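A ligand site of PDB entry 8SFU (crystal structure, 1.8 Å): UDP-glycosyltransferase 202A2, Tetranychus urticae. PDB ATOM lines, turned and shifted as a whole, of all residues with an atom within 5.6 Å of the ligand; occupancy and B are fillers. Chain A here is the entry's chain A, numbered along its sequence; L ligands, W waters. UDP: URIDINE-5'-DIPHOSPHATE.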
ATOM      1  N   PRO A  23      15.178  -9.138  17.913  1.00  0.00           N
ATOM      2  CA  PRO A  23      15.272  -7.853  17.212  1.00  0.00           C
ATOM      3  C   PRO A  23      15.303  -8.102  15.690  1.00  0.00           C
ATOM      4  O   PRO A  23      14.739  -7.319  14.971  1.00  0.00           O
ATOM      5  CB  PRO A  23      16.572  -7.239  17.728  1.00  0.00           C
ATOM      6  CG  PRO A  23      16.779  -7.896  19.075  1.00  0.00           C
ATOM      7  CD  PRO A  23      16.222  -9.293  18.930  1.00  0.00           C
ATOM      8  N   GLY A  24      15.955  -9.174  15.259  1.00  0.00           N
ATOM      9  CA  GLY A  24      15.954  -9.575  13.830  1.00  0.00           C
ATOM     10  C   GLY A  24      14.526  -9.710  13.279  1.00  0.00           C
ATOM     11  O   GLY A  24      14.291  -9.202  12.146  1.00  0.00           O
ATOM     12  N   ASN A  27      12.709  -6.507  11.618  1.00  0.00           N
ATOM     13  CA  ASN A  27      13.151  -5.640  10.490  1.00  0.00           C
ATOM     14  C   ASN A  27      12.234  -5.717   9.255  1.00  0.00           C
ATOM     15  O   ASN A  27      11.893  -4.629   8.677  1.00  0.00           O
ATOM     16  CB  ASN A  27      14.548  -6.021  10.032  1.00  0.00           C
ATOM     17  CG  ASN A  27      15.570  -5.611  11.081  1.00  0.00           C
ATOM     18  OD1 ASN A  27      15.304  -4.747  11.907  1.00  0.00           O
ATOM     19  ND2 ASN A  27      16.765  -6.125  10.936  1.00  0.00           N
ATOM     20  N   TYR A 274      34.701  -6.909  10.747  1.00  0.00           N
ATOM     21  CA  TYR A 274      33.616  -6.738  11.722  1.00  0.00           C
ATOM     22  C   TYR A 274      33.304  -8.107  12.295  1.00  0.00           C
ATOM     23  O   TYR A 274      33.194  -9.073  11.533  1.00  0.00           O
ATOM     24  CB  TYR A 274      32.389  -6.137  11.066  1.00  0.00           C
ATOM     25  CG  TYR A 274      31.155  -5.977  11.941  1.00  0.00           C
ATOM     26  CD1 TYR A 274      31.213  -5.488  13.228  1.00  0.00           C
ATOM     27  CD2 TYR A 274      29.929  -6.352  11.485  1.00  0.00           C
ATOM     28  CE1 TYR A 274      30.117  -5.402  14.067  1.00  0.00           C
ATOM     29  CE2 TYR A 274      28.763  -6.217  12.293  1.00  0.00           C
ATOM     30  CZ  TYR A 274      28.857  -5.761  13.595  1.00  0.00           C
ATOM     31  OH  TYR A 274      27.741  -5.637  14.360  1.00  0.00           O
ATOM     32  N   SER A 276      30.589 -10.121  14.807  1.00  0.00           N
ATOM     33  CA  SER A 276      29.338 -10.043  15.587  1.00  0.00           C
ATOM     34  C   SER A 276      28.723 -11.428  15.641  1.00  0.00           C
ATOM     35  O   SER A 276      28.501 -11.999  14.532  1.00  0.00           O
ATOM     36  CB  SER A 276      28.371  -9.082  15.043  1.00  0.00           C
ATOM     37  OG  SER A 276      27.198  -9.156  15.848  1.00  0.00           O
ATOM     38  N   MET A 277      28.423 -11.912  16.837  1.00  0.00           N
ATOM     39  CA  MET A 277      27.667 -13.173  16.967  1.00  0.00           C
ATOM     40  C   MET A 277      26.167 -12.902  17.106  1.00  0.00           C
ATOM     41  O   MET A 277      25.454 -13.873  17.387  1.00  0.00           O
ATOM     42  CB  MET A 277      28.238 -13.965  18.133  1.00  0.00           C
ATOM     43  CG  MET A 277      29.623 -14.477  17.812  1.00  0.00           C
ATOM     44  SD  MET A 277      29.663 -15.712  16.403  1.00  0.00           S
ATOM     45  CE  MET A 277      30.589 -14.768  15.212  1.00  0.00           C
ATOM     46  N   GLY A 278      25.721 -11.667  16.833  1.00  0.00           N
ATOM     47  CA  GLY A 278      24.283 -11.327  16.865  1.00  0.00           C
ATOM     48  C   GLY A 278      23.788 -10.972  18.225  1.00  0.00           C
ATOM     49  O   GLY A 278      24.444 -11.324  19.240  1.00  0.00           O
ATOM     50  N   SER A 279      22.616 -10.299  18.281  1.00  0.00           N
ATOM     51  CA  SER A 279      22.070  -9.745  19.554  1.00  0.00           C
ATOM     52  C   SER A 279      21.955 -10.844  20.613  1.00  0.00           C
ATOM     53  O   SER A 279      22.245 -10.598  21.799  1.00  0.00           O
ATOM     54  CB  SER A 279      20.687  -9.112  19.313  1.00  0.00           C
ATOM     55  OG  SER A 279      20.821  -7.977  18.453  1.00  0.00           O
ATOM     56  N   LEU A 280      21.482 -12.006  20.228  1.00  0.00           N
ATOM     57  CA  LEU A 280      21.116 -13.050  21.205  1.00  0.00           C
ATOM     58  C   LEU A 280      22.322 -13.856  21.666  1.00  0.00           C
ATOM     59  O   LEU A 280      22.540 -13.883  22.881  1.00  0.00           O
ATOM     60  CB  LEU A 280      20.069 -13.972  20.616  1.00  0.00           C
ATOM     61  CG  LEU A 280      18.766 -13.301  20.153  1.00  0.00           C
ATOM     62  CD1 LEU A 280      17.817 -14.403  19.710  1.00  0.00           C
ATOM     63  CD2 LEU A 280      18.175 -12.378  21.218  1.00  0.00           C
ATOM     64  N   SER A 305      31.114  -6.171  17.997  1.00  0.00           N
ATOM     65  CA  SER A 305      29.848  -6.024  18.755  1.00  0.00           C
ATOM     66  C   SER A 305      29.992  -6.911  19.997  1.00  0.00           C
ATOM     67  O   SER A 305      29.988  -8.187  19.885  1.00  0.00           O
ATOM     68  CB  SER A 305      28.643  -6.387  17.856  1.00  0.00           C
ATOM     69  OG  SER A 305      27.451  -6.371  18.656  1.00  0.00           O
ATOM     70  N   LYS A 323      28.960  -2.486  23.034  1.00  0.00           N
ATOM     71  CA  LYS A 323      27.887  -3.478  23.292  1.00  0.00           C
ATOM     72  C   LYS A 323      27.004  -3.616  22.050  1.00  0.00           C
ATOM     73  O   LYS A 323      26.625  -4.758  21.742  1.00  0.00           O
ATOM     74  CB  LYS A 323      27.111  -3.049  24.531  1.00  0.00           C
ATOM     75  CG  LYS A 323      27.934  -3.126  25.799  1.00  0.00           C
ATOM     76  CD  LYS A 323      27.099  -3.058  27.075  1.00  0.00           C
ATOM     77  CE  LYS A 323      26.454  -1.720  27.335  1.00  0.00           C
ATOM     78  NZ  LYS A 323      25.760  -1.812  28.648  1.00  0.00           N
ATOM     79  N   PHE A 324      26.679  -2.494  21.398  1.00  0.00           N
ATOM     80  CA  PHE A 324      25.742  -2.449  20.235  1.00  0.00           C
ATOM     81  C   PHE A 324      26.323  -1.439  19.223  1.00  0.00           C
ATOM     82  O   PHE A 324      26.506  -0.287  19.587  1.00  0.00           O
ATOM     83  CB  PHE A 324      24.321  -2.149  20.754  1.00  0.00           C
ATOM     84  CG  PHE A 324      23.238  -2.327  19.721  1.00  0.00           C
ATOM     85  CD1 PHE A 324      22.784  -3.601  19.401  1.00  0.00           C
ATOM     86  CD2 PHE A 324      22.755  -1.238  19.040  1.00  0.00           C
ATOM     87  CE1 PHE A 324      21.840  -3.776  18.396  1.00  0.00           C
ATOM     88  CE2 PHE A 324      21.770  -1.418  18.066  1.00  0.00           C
ATOM     89  CZ  PHE A 324      21.320  -2.676  17.760  1.00  0.00           C
ATOM     90  N   ILE A 325      26.704  -1.902  18.050  1.00  0.00           N
ATOM     91  CA  ILE A 325      27.425  -1.150  16.982  1.00  0.00           C
ATOM     92  C   ILE A 325      26.338  -0.646  16.000  1.00  0.00           C
ATOM     93  O   ILE A 325      25.354  -1.423  15.794  1.00  0.00           O
ATOM     94  CB  ILE A 325      28.388  -2.154  16.298  1.00  0.00           C
ATOM     95  CG1 ILE A 325      29.533  -2.658  17.180  1.00  0.00           C
ATOM     96  CG2 ILE A 325      28.912  -1.652  14.982  1.00  0.00           C
ATOM     97  CD1 ILE A 325      30.527  -1.635  17.550  1.00  0.00           C
ATOM     98  N   ASN A 326      26.541   0.484  15.311  1.00  0.00           N
ATOM     99  CA  ASN A 326      25.684   0.836  14.149  1.00  0.00           C
ATOM    100  C   ASN A 326      26.077  -0.054  12.951  1.00  0.00           C
ATOM    101  O   ASN A 326      26.933   0.327  12.161  1.00  0.00           O
ATOM    102  CB  ASN A 326      25.820   2.303  13.756  1.00  0.00           C
ATOM    103  CG  ASN A 326      24.803   2.665  12.704  1.00  0.00           C
ATOM    104  OD1 ASN A 326      24.276   1.808  12.007  1.00  0.00           O
ATOM    105  ND2 ASN A 326      24.451   3.941  12.654  1.00  0.00           N
ATOM    106  N   GLN A 327      25.500  -1.252  12.851  1.00  0.00           N
ATOM    107  CA  GLN A 327      26.021  -2.320  11.984  1.00  0.00           C
ATOM    108  C   GLN A 327      25.857  -1.914  10.515  1.00  0.00           C
ATOM    109  O   GLN A 327      26.755  -2.160   9.681  1.00  0.00           O
ATOM    110  CB  GLN A 327      25.269  -3.606  12.341  1.00  0.00           C
ATOM    111  CG  GLN A 327      25.483  -4.719  11.345  1.00  0.00           C
ATOM    112  CD  GLN A 327      25.161  -6.081  11.885  1.00  0.00           C
ATOM    113  OE1 GLN A 327      25.488  -6.425  12.994  1.00  0.00           O
ATOM    114  NE2 GLN A 327      24.447  -6.884  11.111  1.00  0.00           N
ATOM    115  N   VAL A 328      24.701  -1.326  10.166  1.00  0.00           N
ATOM    116  CA  VAL A 328      24.454  -0.964   8.743  1.00  0.00           C
ATOM    117  C   VAL A 328      25.377   0.183   8.314  1.00  0.00           C
ATOM    118  O   VAL A 328      25.836   0.176   7.184  1.00  0.00           O
ATOM    119  CB  VAL A 328      22.953  -0.630   8.518  1.00  0.00           C
ATOM    120  CG1 VAL A 328      22.693  -0.096   7.106  1.00  0.00           C
ATOM    121  CG2 VAL A 328      22.100  -1.883   8.763  1.00  0.00           C
ATOM    122  N   HIS A 340      27.521 -14.983  13.024  1.00  0.00           N
ATOM    123  CA  HIS A 340      26.847 -16.239  13.464  1.00  0.00           C
ATOM    124  C   HIS A 340      25.998 -16.799  12.333  1.00  0.00           C
ATOM    125  O   HIS A 340      25.562 -17.955  12.474  1.00  0.00           O
ATOM    126  CB  HIS A 340      25.988 -15.968  14.709  1.00  0.00           C
ATOM    127  CG  HIS A 340      24.880 -15.008  14.489  1.00  0.00           C
ATOM    128  ND1 HIS A 340      25.102 -13.773  14.017  1.00  0.00           N
ATOM    129  CD2 HIS A 340      23.536 -15.122  14.675  1.00  0.00           C
ATOM    130  CE1 HIS A 340      23.956 -13.091  13.941  1.00  0.00           C
ATOM    131  NE2 HIS A 340      22.946 -13.890  14.361  1.00  0.00           N
ATOM    132  N   GLY A 341      25.777 -16.060  11.246  1.00  0.00           N
ATOM    133  CA  GLY A 341      25.011 -16.555  10.099  1.00  0.00           C
ATOM    134  C   GLY A 341      23.528 -16.279  10.269  1.00  0.00           C
ATOM    135  O   GLY A 341      22.712 -16.918   9.633  1.00  0.00           O
ATOM    136  N   GLY A 342      23.126 -15.375  11.127  1.00  0.00           N
ATOM    137  CA  GLY A 342      21.723 -14.970  11.177  1.00  0.00           C
ATOM    138  C   GLY A 342      21.270 -14.313   9.899  1.00  0.00           C
ATOM    139  O   GLY A 342      22.108 -13.697   9.222  1.00  0.00           O
ATOM    140  N   SER A 343      19.980 -14.403   9.554  1.00  0.00           N
ATOM    141  CA  SER A 343      19.447 -13.908   8.266  1.00  0.00           C
ATOM    142  C   SER A 343      19.596 -12.403   8.113  1.00  0.00           C
ATOM    143  O   SER A 343      19.888 -11.952   6.979  1.00  0.00           O
ATOM    144  CB  SER A 343      17.995 -14.332   8.059  1.00  0.00           C
ATOM    145  OG  SER A 343      17.962 -15.753   7.917  1.00  0.00           O
ATOM    146  N   ASN A 344      19.313 -11.634   9.156  1.00  0.00           N
ATOM    147  CA  ASN A 344      19.470 -10.148   9.053  1.00  0.00           C
ATOM    148  C   ASN A 344      20.921  -9.793   8.762  1.00  0.00           C
ATOM    149  O   ASN A 344      21.186  -8.986   7.840  1.00  0.00           O
ATOM    150  CB  ASN A 344      18.900  -9.436  10.271  1.00  0.00           C
ATOM    151  CG  ASN A 344      17.398  -9.575  10.268  1.00  0.00           C
ATOM    152  OD1 ASN A 344      16.710  -8.886   9.513  1.00  0.00           O
ATOM    153  ND2 ASN A 344      16.882 -10.508  11.051  1.00  0.00           N
ATOM    154  N   SER A 345      21.834 -10.409   9.467  1.00  0.00           N
ATOM    155  CA  SER A 345      23.273 -10.101   9.279  1.00  0.00           C
ATOM    156  C   SER A 345      23.694 -10.547   7.876  1.00  0.00           C
ATOM    157  O   SER A 345      24.500  -9.873   7.244  1.00  0.00           O
ATOM    158  CB  SER A 345      24.121 -10.714  10.330  1.00  0.00           C
ATOM    159  OG  SER A 345      24.034  -9.962  11.508  1.00  0.00           O
ATOM    160  N   LEU A 346      23.208 -11.706   7.428  1.00  0.00           N
ATOM    161  CA  LEU A 346      23.507 -12.240   6.072  1.00  0.00           C
ATOM    162  C   LEU A 346      23.073 -11.222   4.988  1.00  0.00           C
ATOM    163  O   LEU A 346      23.880 -10.851   4.095  1.00  0.00           O
ATOM    164  CB  LEU A 346      22.733 -13.548   5.903  1.00  0.00           C
ATOM    165  CG  LEU A 346      22.768 -14.170   4.529  1.00  0.00           C
ATOM    166  CD1 LEU A 346      24.192 -14.607   4.248  1.00  0.00           C
ATOM    167  CD2 LEU A 346      21.830 -15.348   4.490  1.00  0.00           C
ATOM    168  N   GLU A 348      22.386  -7.998   5.298  1.00  0.00           N
ATOM    169  CA  GLU A 348      23.081  -6.696   5.468  1.00  0.00           C
ATOM    170  C   GLU A 348      24.484  -6.833   4.900  1.00  0.00           C
ATOM    171  O   GLU A 348      24.952  -5.929   4.166  1.00  0.00           O
ATOM    172  CB  GLU A 348      23.032  -6.248   6.919  1.00  0.00           C
ATOM    173  CG  GLU A 348      21.614  -5.812   7.303  1.00  0.00           C
ATOM    174  CD  GLU A 348      21.379  -5.677   8.805  1.00  0.00           C
ATOM    175  OE1 GLU A 348      22.374  -5.647   9.580  1.00  0.00           O
ATOM    176  OE2 GLU A 348      20.231  -5.488   9.218  1.00  0.00           O
ATOM    177  N   GLN A 365      20.547 -20.600  11.463  1.00  0.00           N
ATOM    178  CA  GLN A 365      21.926 -20.164  11.180  1.00  0.00           C
ATOM    179  C   GLN A 365      22.740 -21.275  10.538  1.00  0.00           C
ATOM    180  O   GLN A 365      23.619 -20.970   9.675  1.00  0.00           O
ATOM    181  CB  GLN A 365      22.624 -19.712  12.468  1.00  0.00           C
ATOM    182  CG  GLN A 365      21.952 -18.483  13.064  1.00  0.00           C
ATOM    183  CD  GLN A 365      22.245 -18.387  14.542  1.00  0.00           C
ATOM    184  OE1 GLN A 365      23.188 -19.000  15.045  1.00  0.00           O
ATOM    185  NE2 GLN A 365      21.393 -17.668  15.287  1.00  0.00           N
HETATM  186  N1  UDP L   1      22.497  -4.971  15.093  1.00  0.00           N
HETATM  187  C2  UDP L   1      23.196  -3.783  15.144  1.00  0.00           C
HETATM  188  N3  UDP L   1      24.311  -3.804  15.953  1.00  0.00           N
HETATM  189  C4  UDP L   1      24.778  -4.874  16.686  1.00  0.00           C
HETATM  190  C5  UDP L   1      24.010  -6.069  16.572  1.00  0.00           C
HETATM  191  C6  UDP L   1      22.914  -6.078  15.792  1.00  0.00           C
HETATM  192  O2  UDP L   1      22.852  -2.781  14.534  1.00  0.00           O
HETATM  193  O4  UDP L   1      25.802  -4.732  17.362  1.00  0.00           O
HETATM  194  C1' UDP L   1      21.300  -5.006  14.231  1.00  0.00           C
HETATM  195  C2' UDP L   1      21.542  -5.678  12.887  1.00  0.00           C
HETATM  196  O2' UDP L   1      22.070  -4.735  11.970  1.00  0.00           O
HETATM  197  C3' UDP L   1      20.138  -6.158  12.522  1.00  0.00           C
HETATM  198  C4' UDP L   1      19.524  -6.503  13.895  1.00  0.00           C
HETATM  199  O4' UDP L   1      20.305  -5.771  14.875  1.00  0.00           O
HETATM  200  O3' UDP L   1      19.369  -5.145  11.870  1.00  0.00           O
HETATM  201  C5' UDP L   1      19.536  -7.968  14.251  1.00  0.00           C
HETATM  202  O5' UDP L   1      20.917  -8.429  14.231  1.00  0.00           O
HETATM  203  PA  UDP L   1      21.202  -9.964  14.568  1.00  0.00           P
HETATM  204  O1A UDP L   1      20.847 -10.228  15.991  1.00  0.00           O
HETATM  205  O2A UDP L   1      22.570 -10.318  14.091  1.00  0.00           O
HETATM  206  O3A UDP L   1      20.128 -10.662  13.614  1.00  0.00           O
HETATM  207  PB  UDP L   1      20.176 -12.043  12.800  1.00  0.00           P
HETATM  208  O1B UDP L   1      21.330 -11.896  11.844  1.00  0.00           O
HETATM  209  O2B UDP L   1      20.403 -13.124  13.813  1.00  0.00           O
HETATM  210  O3B UDP L   1      18.849 -12.172  12.095  1.00  0.00           O
HETATM  211  O   HOH W   1      18.136 -10.803  16.584  1.00  0.00           O
HETATM  212  O   HOH W   2      20.416  -2.685  11.841  1.00  0.00           O
HETATM  213  O   HOH W   3      19.480 -15.816  13.884  1.00  0.00           O
HETATM  214  O   HOH W   4      25.011  -8.765  14.261  1.00  0.00           O
HETATM  215  O   HOH W   5      20.861 -12.814  17.152  1.00  0.00           O
HETATM  216  O   HOH W   6      22.357  -0.777  11.932  1.00  0.00           O
HETATM  217  O   HOH W   7      22.393  -0.020  14.913  1.00  0.00           O
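Water W7 bridges O2 of the ligand (2.8 Å) and O of Ile 325 (3.4 Å).
Water W1 bridges O1A of the ligand (2.8 Å) and N of Gly 24 (3.0 Å).
Water W5 lies within hydrogen-bond range of O1A of the ligand (2.8 Å), N of Leu 280 (3.2 Å) and N of Ser 279 (3.3 Å).
Water W3 lies within hydrogen-bond range of O2B of the ligand (2.8 Å) and NE2 of Gln 365 (3.0 Å).
Water W4 lies within hydrogen-bond range of the side-chain amide oxygen of Gln 327 (2.7 Å), the side-chain hydroxyl of Ser 276 (2.7 Å), an oxygen (O2A) of the ligand (2.9 Å) and the side-chain hydroxyl of Ser 345 (3.2 Å).
Water W6 lies within hydrogen-bond range of N of Val 328 (3.0 Å), OD1 of Asn 326 (3.2 Å), N of Gln 327 (3.3 Å) and O2 of the ligand (3.3 Å).
A ring nitrogen (ND1) of His 340 sits close to the backbone carbonyl oxygen (O) of Met 277.
The backbone carbonyl oxygen (O) of Gly 24 sits close to the side-chain amide nitrogen (ND2) of Asn 344.
The side-chain amide oxygen of Asn 344 is in hydrogen-bond range of the side-chain amide nitrogen of Asn 27, at 3.1 Å.
O of Ser 276 is in hydrogen-bond range of N of His 340, at 3.5 Å.
NE2 of Gln 327 sits at hydrogen-bond distance from OE1 of Glu 348, at 2.9 Å.
N of Gly 278 is in hydrogen-bond range of OG of Ser 276 (3.1 Å).
NE2 of Gln 327 lies within hydrogen-bond range of OG of Ser 345 (3.1 Å).
OE1 of Gln 327 sits at hydrogen-bond distance from OH of Tyr 274 (2.8 Å).
The backbone NH (N) of Asn 344 is in hydrogen-bond range of an oxygen (O3B) of the ligand, 3.0 Å away.
O of Ile 325 lies within hydrogen-bond range of N3 of the ligand (2.6 Å).
The side-chain hydroxyl of Ser 345 lies within hydrogen-bond range of an oxygen (O2A) of the ligand (3.0 Å).
A ring nitrogen (NE2) of His 340 lies within hydrogen-bond range of an oxygen (O2B) of the ligand, 2.7 Å away.
The side-chain carboxylate of Glu 348 sits at hydrogen-bond distance from an oxygen (O2') of the ligand (2.6 Å).
The backbone NH of Ile 325 lies within hydrogen-bond range of an oxygen (O4) of the ligand, at 3.0 Å.
The backbone NH (N) of Gln 327 lies close to an oxygen (O2) of the ligand (3.5 Å).
ND2 of Asn 27 is in hydrogen-bond range of O3' of the ligand (2.9 Å).
The side-chain amide nitrogen of Gln 327 sits at hydrogen-bond distance from an oxygen (O2') of the ligand (3.3 Å).
OG of Ser 279 is in hydrogen-bond range of O1A of the ligand (3.3 Å).
The backbone NH of Ser 345 lies within hydrogen-bond range of an oxygen (O1B) of the ligand (2.8 Å).
An oxygen (O1A) of the ligand sits at hydrogen-bond distance from the backbone NH (N) of Ser 279, at 2.9 Å.
ND2 of Asn 344 lies within hydrogen-bond range of O3B of the ligand, at 2.8 Å.
The side-chain hydroxyl (OG) of Ser 305 sits at hydrogen-bond distance from an oxygen (O4) of the ligand, 2.7 Å away.
An oxygen (O1B) of the ligand lies close to the backbone carbonyl oxygen (O) of Gly 342, at 3.3 Å.
N of Gly 24 touches C5' of the ligand, 3.9 Å away.
Tyr 274 touches the ligand (OH to O4, 3.7 Å).
Gly 278 touches the ligand.
Phe 324 touches the ligand (CZ to C2, 3.4 Å).
Ser 343 touches the ligand (N to O3B, 3.6 Å).
Hydrophobic or aromatic side chains within 4 Å of the ligand: Phe 324, Ile 325 and His 340.
The nearest printed residue that does not touch the ligand is Val 328 (4.3 Å).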
